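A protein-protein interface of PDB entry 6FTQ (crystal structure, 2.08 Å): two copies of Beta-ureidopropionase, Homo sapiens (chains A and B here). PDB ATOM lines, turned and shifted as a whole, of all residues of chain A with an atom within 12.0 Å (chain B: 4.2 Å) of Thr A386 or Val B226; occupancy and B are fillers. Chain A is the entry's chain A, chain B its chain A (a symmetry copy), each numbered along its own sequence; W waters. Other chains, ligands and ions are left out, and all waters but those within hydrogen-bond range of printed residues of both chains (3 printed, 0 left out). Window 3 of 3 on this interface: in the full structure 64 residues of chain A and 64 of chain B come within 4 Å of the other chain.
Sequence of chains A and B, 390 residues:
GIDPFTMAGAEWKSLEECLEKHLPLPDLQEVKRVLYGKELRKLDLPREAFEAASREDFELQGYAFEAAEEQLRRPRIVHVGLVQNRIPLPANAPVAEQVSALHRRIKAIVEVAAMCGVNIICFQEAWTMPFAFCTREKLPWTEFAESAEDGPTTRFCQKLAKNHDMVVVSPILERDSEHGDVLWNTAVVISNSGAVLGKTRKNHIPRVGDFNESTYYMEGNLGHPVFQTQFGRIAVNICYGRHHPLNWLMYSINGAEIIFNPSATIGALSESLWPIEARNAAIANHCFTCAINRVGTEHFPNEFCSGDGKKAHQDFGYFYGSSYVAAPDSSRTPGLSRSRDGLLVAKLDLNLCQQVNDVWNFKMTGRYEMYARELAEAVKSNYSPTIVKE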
ATOM      1  N   MET A 370     -30.094   2.730 -16.616  1.00  0.00           N
ATOM      2  CA  MET A 370     -28.821   2.055 -16.816  1.00  0.00           C
ATOM      3  C   MET A 370     -28.670   1.517 -18.253  1.00  0.00           C
ATOM      4  O   MET A 370     -27.620   1.695 -18.855  1.00  0.00           O
ATOM      5  CB  MET A 370     -28.639   0.924 -15.786  1.00  0.00           C
ATOM      6  CG  MET A 370     -27.278   0.251 -15.823  1.00  0.00           C
ATOM      7  SD  MET A 370     -27.282  -1.343 -14.980  1.00  0.00           S
ATOM      8  CE  MET A 370     -28.308  -2.303 -16.082  1.00  0.00           C
ATOM      9  N   TYR A 371     -29.706   0.866 -18.789  1.00  0.00           N
ATOM     10  CA  TYR A 371     -29.647   0.369 -20.168  1.00  0.00           C
ATOM     11  C   TYR A 371     -29.554   1.478 -21.223  1.00  0.00           C
ATOM     12  O   TYR A 371     -28.853   1.315 -22.216  1.00  0.00           O
ATOM     13  CB  TYR A 371     -30.805  -0.599 -20.472  1.00  0.00           C
ATOM     14  CG  TYR A 371     -30.580  -1.920 -19.772  1.00  0.00           C
ATOM     15  CD1 TYR A 371     -29.601  -2.804 -20.229  1.00  0.00           C
ATOM     16  CD2 TYR A 371     -31.297  -2.264 -18.625  1.00  0.00           C
ATOM     17  CE1 TYR A 371     -29.362  -4.011 -19.587  1.00  0.00           C
ATOM     18  CE2 TYR A 371     -31.061  -3.466 -17.968  1.00  0.00           C
ATOM     19  CZ  TYR A 371     -30.080  -4.335 -18.443  1.00  0.00           C
ATOM     20  OH  TYR A 371     -29.832  -5.537 -17.812  1.00  0.00           O
ATOM     21  N   ARG A 373     -27.990   4.280 -20.851  1.00  0.00           N
ATOM     22  CA  ARG A 373     -26.557   4.619 -20.812  1.00  0.00           C
ATOM     23  C   ARG A 373     -25.670   3.558 -21.490  1.00  0.00           C
ATOM     24  O   ARG A 373     -24.873   3.899 -22.365  1.00  0.00           O
ATOM     25  CB  ARG A 373     -26.098   4.938 -19.376  1.00  0.00           C
ATOM     26  CG  ARG A 373     -26.770   6.196 -18.824  1.00  0.00           C
ATOM     27  CD  ARG A 373     -26.184   6.705 -17.501  1.00  0.00           C
ATOM     28  NE  ARG A 373     -26.776   6.044 -16.325  1.00  0.00           N
ATOM     29  CZ  ARG A 373     -26.318   4.932 -15.731  1.00  0.00           C
ATOM     30  NH1 ARG A 373     -25.218   4.297 -16.166  1.00  0.00           N
ATOM     31  NH2 ARG A 373     -26.967   4.446 -14.669  1.00  0.00           N
ATOM     32  N   GLU A 374     -25.852   2.284 -21.145  1.00  0.00           N
ATOM     33  CA  GLU A 374     -25.060   1.206 -21.758  1.00  0.00           C
ATOM     34  C   GLU A 374     -25.255   1.076 -23.281  1.00  0.00           C
ATOM     35  O   GLU A 374     -24.280   0.842 -24.009  1.00  0.00           O
ATOM     36  CB  GLU A 374     -25.337  -0.155 -21.097  1.00  0.00           C
ATOM     37  CG  GLU A 374     -24.717  -0.334 -19.732  1.00  0.00           C
ATOM     38  CD  GLU A 374     -24.774  -1.772 -19.234  1.00  0.00           C
ATOM     39  OE1 GLU A 374     -24.340  -2.697 -19.949  1.00  0.00           O
ATOM     40  OE2 GLU A 374     -25.227  -1.973 -18.093  1.00  0.00           O
ATOM     41  N   LEU A 375     -26.499   1.210 -23.746  1.00  0.00           N
ATOM     42  CA  LEU A 375     -26.790   1.150 -25.188  1.00  0.00           C
ATOM     43  C   LEU A 375     -26.163   2.312 -25.957  1.00  0.00           C
ATOM     44  O   LEU A 375     -25.591   2.103 -27.023  1.00  0.00           O
ATOM     45  CB  LEU A 375     -28.297   1.127 -25.490  1.00  0.00           C
ATOM     46  CG  LEU A 375     -28.979  -0.192 -25.807  1.00  0.00           C
ATOM     47  CD1 LEU A 375     -30.390   0.096 -26.299  1.00  0.00           C
ATOM     48  CD2 LEU A 375     -28.228  -1.010 -26.842  1.00  0.00           C
ATOM     49  N   ALA A 376     -26.288   3.522 -25.420  1.00  0.00           N
ATOM     50  CA  ALA A 376     -25.675   4.714 -26.034  1.00  0.00           C
ATOM     51  C   ALA A 376     -24.164   4.547 -26.199  1.00  0.00           C
ATOM     52  O   ALA A 376     -23.613   4.897 -27.242  1.00  0.00           O
ATOM     53  CB  ALA A 376     -25.977   5.973 -25.225  1.00  0.00           C
ATOM     54  N   GLU A 377     -23.520   4.000 -25.172  1.00  0.00           N
ATOM     55  CA  GLU A 377     -22.089   3.736 -25.209  1.00  0.00           C
ATOM     56  C   GLU A 377     -21.783   2.670 -26.253  1.00  0.00           C
ATOM     57  O   GLU A 377     -20.849   2.827 -27.046  1.00  0.00           O
ATOM     58  CB  GLU A 377     -21.578   3.322 -23.822  1.00  0.00           C
ATOM     59  CG  GLU A 377     -20.060   3.245 -23.670  1.00  0.00           C
ATOM     60  CD  GLU A 377     -19.302   4.543 -23.987  1.00  0.00           C
ATOM     61  OE1 GLU A 377     -19.868   5.668 -23.919  1.00  0.00           O
ATOM     62  OE2 GLU A 377     -18.097   4.428 -24.313  1.00  0.00           O
ATOM     63  N   ALA A 378     -22.602   1.621 -26.288  1.00  0.00           N
ATOM     64  CA  ALA A 378     -22.414   0.523 -27.242  1.00  0.00           C
ATOM     65  C   ALA A 378     -22.553   0.905 -28.719  1.00  0.00           C
ATOM     66  O   ALA A 378     -21.834   0.375 -29.552  1.00  0.00           O
ATOM     67  CB  ALA A 378     -23.314  -0.661 -26.905  1.00  0.00           C
ATOM     68  N   VAL A 379     -23.459   1.819 -29.040  1.00  0.00           N
ATOM     69  CA  VAL A 379     -23.669   2.221 -30.451  1.00  0.00           C
ATOM     70  C   VAL A 379     -22.558   3.112 -31.043  1.00  0.00           C
ATOM     71  O   VAL A 379     -22.450   3.220 -32.265  1.00  0.00           O
ATOM     72  CB  VAL A 379     -25.045   2.911 -30.692  1.00  0.00           C
ATOM     73  CG1 VAL A 379     -26.190   1.960 -30.374  1.00  0.00           C
ATOM     74  CG2 VAL A 379     -25.184   4.215 -29.910  1.00  0.00           C
ATOM     75  N   LYS A 380     -21.757   3.756 -30.195  1.00  0.00           N
ATOM     76  CA  LYS A 380     -20.663   4.611 -30.680  1.00  0.00           C
ATOM     77  C   LYS A 380     -19.689   3.874 -31.608  1.00  0.00           C
ATOM     78  O   LYS A 380     -19.380   2.687 -31.412  1.00  0.00           O
ATOM     79  CB  LYS A 380     -19.883   5.235 -29.524  1.00  0.00           C
ATOM     80  CG  LYS A 380     -20.663   6.278 -28.747  1.00  0.00           C
ATOM     81  CD  LYS A 380     -19.779   6.902 -27.682  1.00  0.00           C
ATOM     82  CE  LYS A 380     -20.595   7.644 -26.638  1.00  0.00           C
ATOM     83  NZ  LYS A 380     -19.709   8.190 -25.568  1.00  0.00           N
ATOM     84  N   ASN A 382     -16.522   4.139 -32.015  1.00  0.00           N
ATOM     85  CA  ASN A 382     -15.278   3.700 -31.344  1.00  0.00           C
ATOM     86  C   ASN A 382     -15.521   2.749 -30.133  1.00  0.00           C
ATOM     87  O   ASN A 382     -14.657   2.620 -29.256  1.00  0.00           O
ATOM     88  CB  ASN A 382     -14.435   4.933 -30.935  1.00  0.00           C
ATOM     89  CG  ASN A 382     -15.240   5.980 -30.164  1.00  0.00           C
ATOM     90  OD1 ASN A 382     -15.948   5.665 -29.200  1.00  0.00           O
ATOM     91  ND2 ASN A 382     -15.150   7.230 -30.601  1.00  0.00           N
ATOM     92  N   TYR A 383     -16.669   2.066 -30.094  1.00  0.00           N
ATOM     93  CA  TYR A 383     -17.002   1.195 -28.956  1.00  0.00           C
ATOM     94  C   TYR A 383     -16.188  -0.107 -28.931  1.00  0.00           C
ATOM     95  O   TYR A 383     -16.287  -0.936 -29.845  1.00  0.00           O
ATOM     96  CB  TYR A 383     -18.483   0.851 -28.964  1.00  0.00           C
ATOM     97  CG  TYR A 383     -18.944   0.055 -27.757  1.00  0.00           C
ATOM     98  CD1 TYR A 383     -18.888   0.606 -26.468  1.00  0.00           C
ATOM     99  CD2 TYR A 383     -19.464  -1.242 -27.899  1.00  0.00           C
ATOM    100  CE1 TYR A 383     -19.332  -0.109 -25.354  1.00  0.00           C
ATOM    101  CE2 TYR A 383     -19.913  -1.967 -26.788  1.00  0.00           C
ATOM    102  CZ  TYR A 383     -19.848  -1.396 -25.518  1.00  0.00           C
ATOM    103  OH  TYR A 383     -20.295  -2.090 -24.420  1.00  0.00           O
ATOM    104  N   SER A 384     -15.389  -0.268 -27.877  1.00  0.00           N
ATOM    105  CA  SER A 384     -14.696  -1.521 -27.579  1.00  0.00           C
ATOM    106  C   SER A 384     -15.538  -2.230 -26.519  1.00  0.00           C
ATOM    107  O   SER A 384     -15.692  -1.706 -25.409  1.00  0.00           O
ATOM    108  CB  SER A 384     -13.286  -1.245 -27.053  1.00  0.00           C
ATOM    109  OG  SER A 384     -13.331  -0.415 -25.904  1.00  0.00           O
ATOM    110  N   PRO A 385     -16.121  -3.401 -26.855  1.00  0.00           N
ATOM    111  CA  PRO A 385     -16.998  -4.070 -25.880  1.00  0.00           C
ATOM    112  C   PRO A 385     -16.330  -4.455 -24.546  1.00  0.00           C
ATOM    113  O   PRO A 385     -15.104  -4.635 -24.478  1.00  0.00           O
ATOM    114  CB  PRO A 385     -17.454  -5.332 -26.626  1.00  0.00           C
ATOM    115  CG  PRO A 385     -17.332  -4.995 -28.069  1.00  0.00           C
ATOM    116  CD  PRO A 385     -16.151  -4.076 -28.171  1.00  0.00           C
ATOM    117  N   THR A 386     -17.167  -4.570 -23.512  1.00  0.00           N
ATOM    118  CA  THR A 386     -16.773  -5.020 -22.158  1.00  0.00           C
ATOM    119  C   THR A 386     -16.355  -6.510 -22.179  1.00  0.00           C
ATOM    120  O   THR A 386     -17.162  -7.390 -21.859  1.00  0.00           O
ATOM    121  CB  THR A 386     -17.945  -4.775 -21.137  1.00  0.00           C
ATOM    122  OG1 THR A 386     -18.372  -3.407 -21.221  1.00  0.00           O
ATOM    123  CG2 THR A 386     -17.531  -5.057 -19.688  1.00  0.00           C
ATOM    124  N   ILE A 387     -15.092  -6.771 -22.548  1.00  0.00           N
ATOM    125  CA  ILE A 387     -14.591  -8.151 -22.730  1.00  0.00           C
ATOM    126  C   ILE A 387     -13.330  -8.458 -21.908  1.00  0.00           C
ATOM    127  O   ILE A 387     -12.321  -7.755 -22.005  1.00  0.00           O
ATOM    128  CB  ILE A 387     -14.386  -8.529 -24.225  1.00  0.00           C
ATOM    129  CG1 ILE A 387     -14.150 -10.047 -24.359  1.00  0.00           C
ATOM    130  CG2 ILE A 387     -13.241  -7.740 -24.865  1.00  0.00           C
ATOM    131  CD1 ILE A 387     -14.090 -10.555 -25.786  1.00  0.00           C
ATOM    132  N   VAL A 388     -13.402  -9.543 -21.131  1.00  0.00           N
ATOM    133  CA  VAL A 388     -12.347  -9.950 -20.207  1.00  0.00           C
ATOM    134  C   VAL A 388     -11.562 -11.147 -20.789  1.00  0.00           C
ATOM    135  O   VAL A 388     -12.149 -12.108 -21.292  1.00  0.00           O
ATOM    136  CB  VAL A 388     -12.937 -10.320 -18.823  1.00  0.00           C
ATOM    137  CG1 VAL A 388     -11.831 -10.380 -17.773  1.00  0.00           C
ATOM    138  CG2 VAL A 388     -14.027  -9.336 -18.399  1.00  0.00           C
ATOM    139  N   LYS A 389     -10.231 -11.065 -20.711  1.00  0.00           N
ATOM    140  CA  LYS A 389      -9.330 -12.075 -21.268  1.00  0.00           C
ATOM    141  C   LYS A 389      -8.263 -12.456 -20.224  1.00  0.00           C
ATOM    142  O   LYS A 389      -8.037 -11.710 -19.263  1.00  0.00           O
ATOM    143  CB  LYS A 389      -8.688 -11.535 -22.559  1.00  0.00           C
ATOM    144  CG  LYS A 389      -8.254 -12.615 -23.545  1.00  0.00           C
ATOM    145  CD  LYS A 389      -7.699 -12.027 -24.836  1.00  0.00           C
ATOM    146  CE  LYS A 389      -7.228 -13.114 -25.795  1.00  0.00           C
ATOM    147  NZ  LYS A 389      -6.042 -13.870 -25.296  1.00  0.00           N
ATOM    148  N   GLU A 390      -7.635 -13.621 -20.396  1.00  0.00           N
ATOM    149  CA  GLU A 390      -6.586 -14.082 -19.479  1.00  0.00           C
ATOM    150  C   GLU A 390      -5.276 -13.333 -19.751  1.00  0.00           C
ATOM    151  O   GLU A 390      -5.092 -12.734 -20.805  1.00  0.00           O
ATOM    152  CB  GLU A 390      -6.364 -15.602 -19.595  1.00  0.00           C
ATOM    153  CG  GLU A 390      -5.721 -16.216 -18.352  1.00  0.00           C
ATOM    154  CD  GLU A 390      -5.523 -17.718 -18.433  1.00  0.00           C
ATOM    155  OE1 GLU A 390      -6.401 -18.431 -18.959  1.00  0.00           O
ATOM    156  OE2 GLU A 390      -4.477 -18.192 -17.946  1.00  0.00           O
ATOM    157  OXT GLU A 390      -4.362 -13.302 -18.929  1.00  0.00           O
ATOM    158  N   HIS B 224     -22.136  -5.538 -18.037  1.00  0.00           N
ATOM    159  CA  HIS B 224     -22.413  -6.754 -18.791  1.00  0.00           C
ATOM    160  C   HIS B 224     -21.125  -7.328 -19.386  1.00  0.00           C
ATOM    161  O   HIS B 224     -20.933  -7.318 -20.607  1.00  0.00           O
ATOM    162  CB  HIS B 224     -23.468  -6.467 -19.861  1.00  0.00           C
ATOM    163  CG  HIS B 224     -24.815  -6.151 -19.284  1.00  0.00           C
ATOM    164  ND1 HIS B 224     -25.171  -4.884 -18.881  1.00  0.00           N
ATOM    165  CD2 HIS B 224     -25.857  -6.952 -18.972  1.00  0.00           C
ATOM    166  CE1 HIS B 224     -26.398  -4.908 -18.388  1.00  0.00           C
ATOM    167  NE2 HIS B 224     -26.836  -6.155 -18.429  1.00  0.00           N
ATOM    168  N   PRO B 225     -20.237  -7.835 -18.513  1.00  0.00           N
ATOM    169  CA  PRO B 225     -18.978  -8.373 -19.007  1.00  0.00           C
ATOM    170  C   PRO B 225     -19.158  -9.669 -19.773  1.00  0.00           C
ATOM    171  O   PRO B 225     -20.100 -10.447 -19.506  1.00  0.00           O
ATOM    172  CB  PRO B 225     -18.158  -8.613 -17.730  1.00  0.00           C
ATOM    173  CG  PRO B 225     -19.180  -8.848 -16.686  1.00  0.00           C
ATOM    174  CD  PRO B 225     -20.358  -7.977 -17.049  1.00  0.00           C
ATOM    175  N   VAL B 226     -18.262  -9.859 -20.729  1.00  0.00           N
ATOM    176  CA  VAL B 226     -18.182 -11.045 -21.540  1.00  0.00           C
ATOM    177  C   VAL B 226     -16.776 -11.576 -21.387  1.00  0.00           C
ATOM    178  O   VAL B 226     -15.826 -10.807 -21.441  1.00  0.00           O
ATOM    179  CB  VAL B 226     -18.532 -10.728 -23.012  1.00  0.00           C
ATOM    180  CG1 VAL B 226     -18.196 -11.911 -23.937  1.00  0.00           C
ATOM    181  CG2 VAL B 226     -20.020 -10.386 -23.109  1.00  0.00           C
ATOM    182  N   PHE B 227     -16.660 -12.887 -21.194  1.00  0.00           N
ATOM    183  CA  PHE B 227     -15.397 -13.535 -20.946  1.00  0.00           C
ATOM    184  C   PHE B 227     -14.961 -14.284 -22.198  1.00  0.00           C
ATOM    185  O   PHE B 227     -15.663 -15.177 -22.679  1.00  0.00           O
ATOM    186  CB  PHE B 227     -15.549 -14.474 -19.748  1.00  0.00           C
ATOM    187  CG  PHE B 227     -15.933 -13.753 -18.492  1.00  0.00           C
ATOM    188  CD1 PHE B 227     -14.949 -13.229 -17.647  1.00  0.00           C
ATOM    189  CD2 PHE B 227     -17.268 -13.546 -18.180  1.00  0.00           C
ATOM    190  CE1 PHE B 227     -15.298 -12.531 -16.496  1.00  0.00           C
ATOM    191  CE2 PHE B 227     -17.630 -12.836 -17.039  1.00  0.00           C
ATOM    192  CZ  PHE B 227     -16.651 -12.335 -16.191  1.00  0.00           C
ATOM    193  N   GLN B 228     -13.828 -13.889 -22.745  1.00  0.00           N
ATOM    194  CA  GLN B 228     -13.235 -14.591 -23.870  1.00  0.00           C
ATOM    195  C   GLN B 228     -12.484 -15.813 -23.355  1.00  0.00           C
ATOM    196  O   GLN B 228     -11.552 -15.664 -22.602  1.00  0.00           O
ATOM    197  CB  GLN B 228     -12.277 -13.673 -24.626  1.00  0.00           C
ATOM    198  CG  GLN B 228     -11.901 -14.207 -26.007  1.00  0.00           C
ATOM    199  CD  GLN B 228     -11.461 -13.099 -26.947  1.00  0.00           C
ATOM    200  OE1 GLN B 228     -12.291 -12.532 -27.685  1.00  0.00           O
ATOM    201  NE2 GLN B 228     -10.170 -12.757 -26.907  1.00  0.00           N
ATOM    202  N   ARG B 233     -16.766 -17.129 -26.354  1.00  0.00           N
ATOM    203  CA  ARG B 233     -17.077 -15.977 -25.549  1.00  0.00           C
ATOM    204  C   ARG B 233     -18.343 -16.276 -24.772  1.00  0.00           C
ATOM    205  O   ARG B 233     -19.381 -16.628 -25.359  1.00  0.00           O
ATOM    206  CB  ARG B 233     -17.228 -14.723 -26.404  1.00  0.00           C
ATOM    207  CG  ARG B 233     -15.944 -14.372 -27.166  1.00  0.00           C
ATOM    208  CD  ARG B 233     -16.106 -13.108 -27.995  1.00  0.00           C
ATOM    209  NE  ARG B 233     -17.118 -13.268 -29.044  1.00  0.00           N
ATOM    210  CZ  ARG B 233     -16.921 -13.849 -30.229  1.00  0.00           C
ATOM    211  NH1 ARG B 233     -17.929 -13.917 -31.097  1.00  0.00           N
ATOM    212  NH2 ARG B 233     -15.738 -14.355 -30.574  1.00  0.00           N
ATOM    213  N   ILE B 234     -18.253 -16.160 -23.448  1.00  0.00           N
ATOM    214  CA  ILE B 234     -19.374 -16.479 -22.570  1.00  0.00           C
ATOM    215  C   ILE B 234     -19.739 -15.318 -21.626  1.00  0.00           C
ATOM    216  O   ILE B 234     -18.928 -14.427 -21.328  1.00  0.00           O
ATOM    217  CB  ILE B 234     -19.119 -17.779 -21.765  1.00  0.00           C
ATOM    218  CG1 ILE B 234     -18.082 -17.586 -20.646  1.00  0.00           C
ATOM    219  CG2 ILE B 234     -18.671 -18.908 -22.687  1.00  0.00           C
ATOM    220  CD1 ILE B 234     -17.832 -18.869 -19.846  1.00  0.00           C
ATOM    221  N   TYR B 251     -25.351  -8.506 -22.954  1.00  0.00           N
ATOM    222  CA  TYR B 251     -24.347  -9.564 -23.054  1.00  0.00           C
ATOM    223  C   TYR B 251     -24.043  -9.956 -24.509  1.00  0.00           C
ATOM    224  O   TYR B 251     -22.876 -10.135 -24.867  1.00  0.00           O
ATOM    225  CB  TYR B 251     -24.741 -10.800 -22.247  1.00  0.00           C
ATOM    226  CG  TYR B 251     -24.720 -10.588 -20.745  1.00  0.00           C
ATOM    227  CD1 TYR B 251     -23.553 -10.212 -20.098  1.00  0.00           C
ATOM    228  CD2 TYR B 251     -25.857 -10.795 -19.975  1.00  0.00           C
ATOM    229  CE1 TYR B 251     -23.513 -10.036 -18.720  1.00  0.00           C
ATOM    230  CE2 TYR B 251     -25.839 -10.612 -18.587  1.00  0.00           C
ATOM    231  CZ  TYR B 251     -24.658 -10.227 -17.969  1.00  0.00           C
ATOM    232  OH  TYR B 251     -24.607 -10.033 -16.608  1.00  0.00           O
ATOM    233  N   ASN B 254     -22.112  -7.180 -26.229  1.00  0.00           N
ATOM    234  CA  ASN B 254     -20.725  -7.199 -25.777  1.00  0.00           C
ATOM    235  C   ASN B 254     -19.958  -8.438 -26.238  1.00  0.00           C
ATOM    236  O   ASN B 254     -18.813  -8.583 -25.890  1.00  0.00           O
ATOM    237  CB  ASN B 254     -20.657  -6.990 -24.248  1.00  0.00           C
ATOM    238  CG  ASN B 254     -21.046  -5.571 -23.841  1.00  0.00           C
ATOM    239  OD1 ASN B 254     -21.031  -4.657 -24.669  1.00  0.00           O
ATOM    240  ND2 ASN B 254     -21.398  -5.376 -22.572  1.00  0.00           N
ATOM    241  N   GLY B 255     -20.606  -9.332 -26.994  1.00  0.00           N
ATOM    242  CA  GLY B 255     -19.934 -10.404 -27.729  1.00  0.00           C
ATOM    243  C   GLY B 255     -20.213 -11.827 -27.265  1.00  0.00           C
ATOM    244  O   GLY B 255     -19.572 -12.749 -27.759  1.00  0.00           O
ATOM    245  N   ALA B 256     -21.152 -12.049 -26.339  1.00  0.00           N
ATOM    246  CA  ALA B 256     -21.350 -13.423 -25.812  1.00  0.00           C
ATOM    247  C   ALA B 256     -21.867 -14.367 -26.898  1.00  0.00           C
ATOM    248  O   ALA B 256     -22.814 -14.025 -27.606  1.00  0.00           O
ATOM    249  CB  ALA B 256     -22.317 -13.420 -24.640  1.00  0.00           C
HETATM  250  O   HOH W   1     -20.649  -3.768 -19.559  1.00  0.00           O
HETATM  251  O   HOH W   2      -9.052 -15.439 -21.903  1.00  0.00           O
HETATM  252  O   HOH W   3     -22.320  -2.811 -21.425  1.00  0.00           O
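The side-chain hydroxyl of Tyr A371 lies within hydrogen-bond range of a ring nitrogen (NE2) of His B224.
ND1 of His B224 lies within hydrogen-bond range of OE1 of Glu A374, at 2.6 Å.
The side-chain hydroxyl (OH) of Tyr A383 is in hydrogen-bond range of the side-chain amide oxygen (OD1) of Asn B254.
N of Val B226 lies within hydrogen-bond range of O of Thr A386, 2.9 Å away.
N of Val A388 sits at hydrogen-bond distance from O of Val B226 (2.8 Å).
The backbone carbonyl oxygen (O) of Val A388 is in hydrogen-bond range of the backbone NH (N) of Gln B228 (2.8 Å).
The backbone carbonyl oxygen (O) of His B224 sits at hydrogen-bond distance from the side-chain amide nitrogen (ND2) of Asn B254 (2.8 Å).
N of Phe B227 sits at hydrogen-bond distance from O of Ile B234 (2.7 Å).
The guanidinium group of Arg B233 is in hydrogen-bond range of the backbone carbonyl oxygen of Gly B255.
Ala A376 touches none of the printed residues of chain B.
Asn A382 touches none of the printed residues of chain B.
Of chain B, only His B224, Pro B225, Val B226 and Asn B254 come within 4 Å of Thr A386.
Printed residues of chain B within 4 Å of Ile A387: Val B226, Gln B228 and Arg B233.
Of the printed residues of chain B, Val A388 touches Val B226, Phe B227 and Gln B228.
Val B226 touches just these residues of chain A: Thr A386, Ile A387 and Val A388.
Ile B234 touches none of the printed residues of chain A.
No residue of chain A comes within 4 Å of Tyr B251.
Of chain A, only Tyr A383, Pro A385 and Thr A386 come within 4 Å of Asn B254.
No residue of chain A comes within 4 Å of Ala B256.
The nearest printed residue of chain B that does not touch Thr A386 is Phe B227 (5.6 Å).
The nearest printed residue of chain A that does not touch His B224 is Ile A387 (6.2 Å).
Water W3 lies within hydrogen-bond range of OE1 of Glu A374 (2.5 Å) and ND2 of Asn B254 (3.0 Å).
Water W2 lies within hydrogen-bond range of O of Gln B228 (2.6 Å) and N of Glu A390 (2.8 Å).
Water W1 lies within hydrogen-bond range of N of His B224 (2.8 Å), OG1 of Thr A386 (2.8 Å) and ND2 of Asn B254 (3.5 Å).
CE1 of His B224 touches CE of Met A370 (3.97 Å).
O of Asn B254 touches CB of Pro A385 (3.6 Å).
Thr A386 touches His B224 (CB to O, 3.96 Å).
CA of Pro B225 touches O of Thr A386, at 3.5 Å.
CB of Thr A386 touches ND2 of Asn B254 (3.8 Å).
O of Val B226 touches CA of Ile A387 (3.2 Å).
Ile A387 touches Gln B228 (CD1 to OE1, 3.3 Å).
Arg B233 touches Ile A387 (CD to CD1, 3.9 Å).
O of Val A388 touches CA of Phe B227, at 3.6 Å.
Gln B228 touches Lys A389.
No position is printed for both chains.
Of the 16 pairs that touch across the chains among the printed residues, none has its exchanged pair printed and touching as well.
Of the 19 printed residues of chain A, 9 touch a printed residue of chain B.
Hydrophobic or aromatic side chains of chain B that line the printed part of chain A: His B224, Val B226 and Phe B227.
Among the printed residues, 16 pairs touch across the chains.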
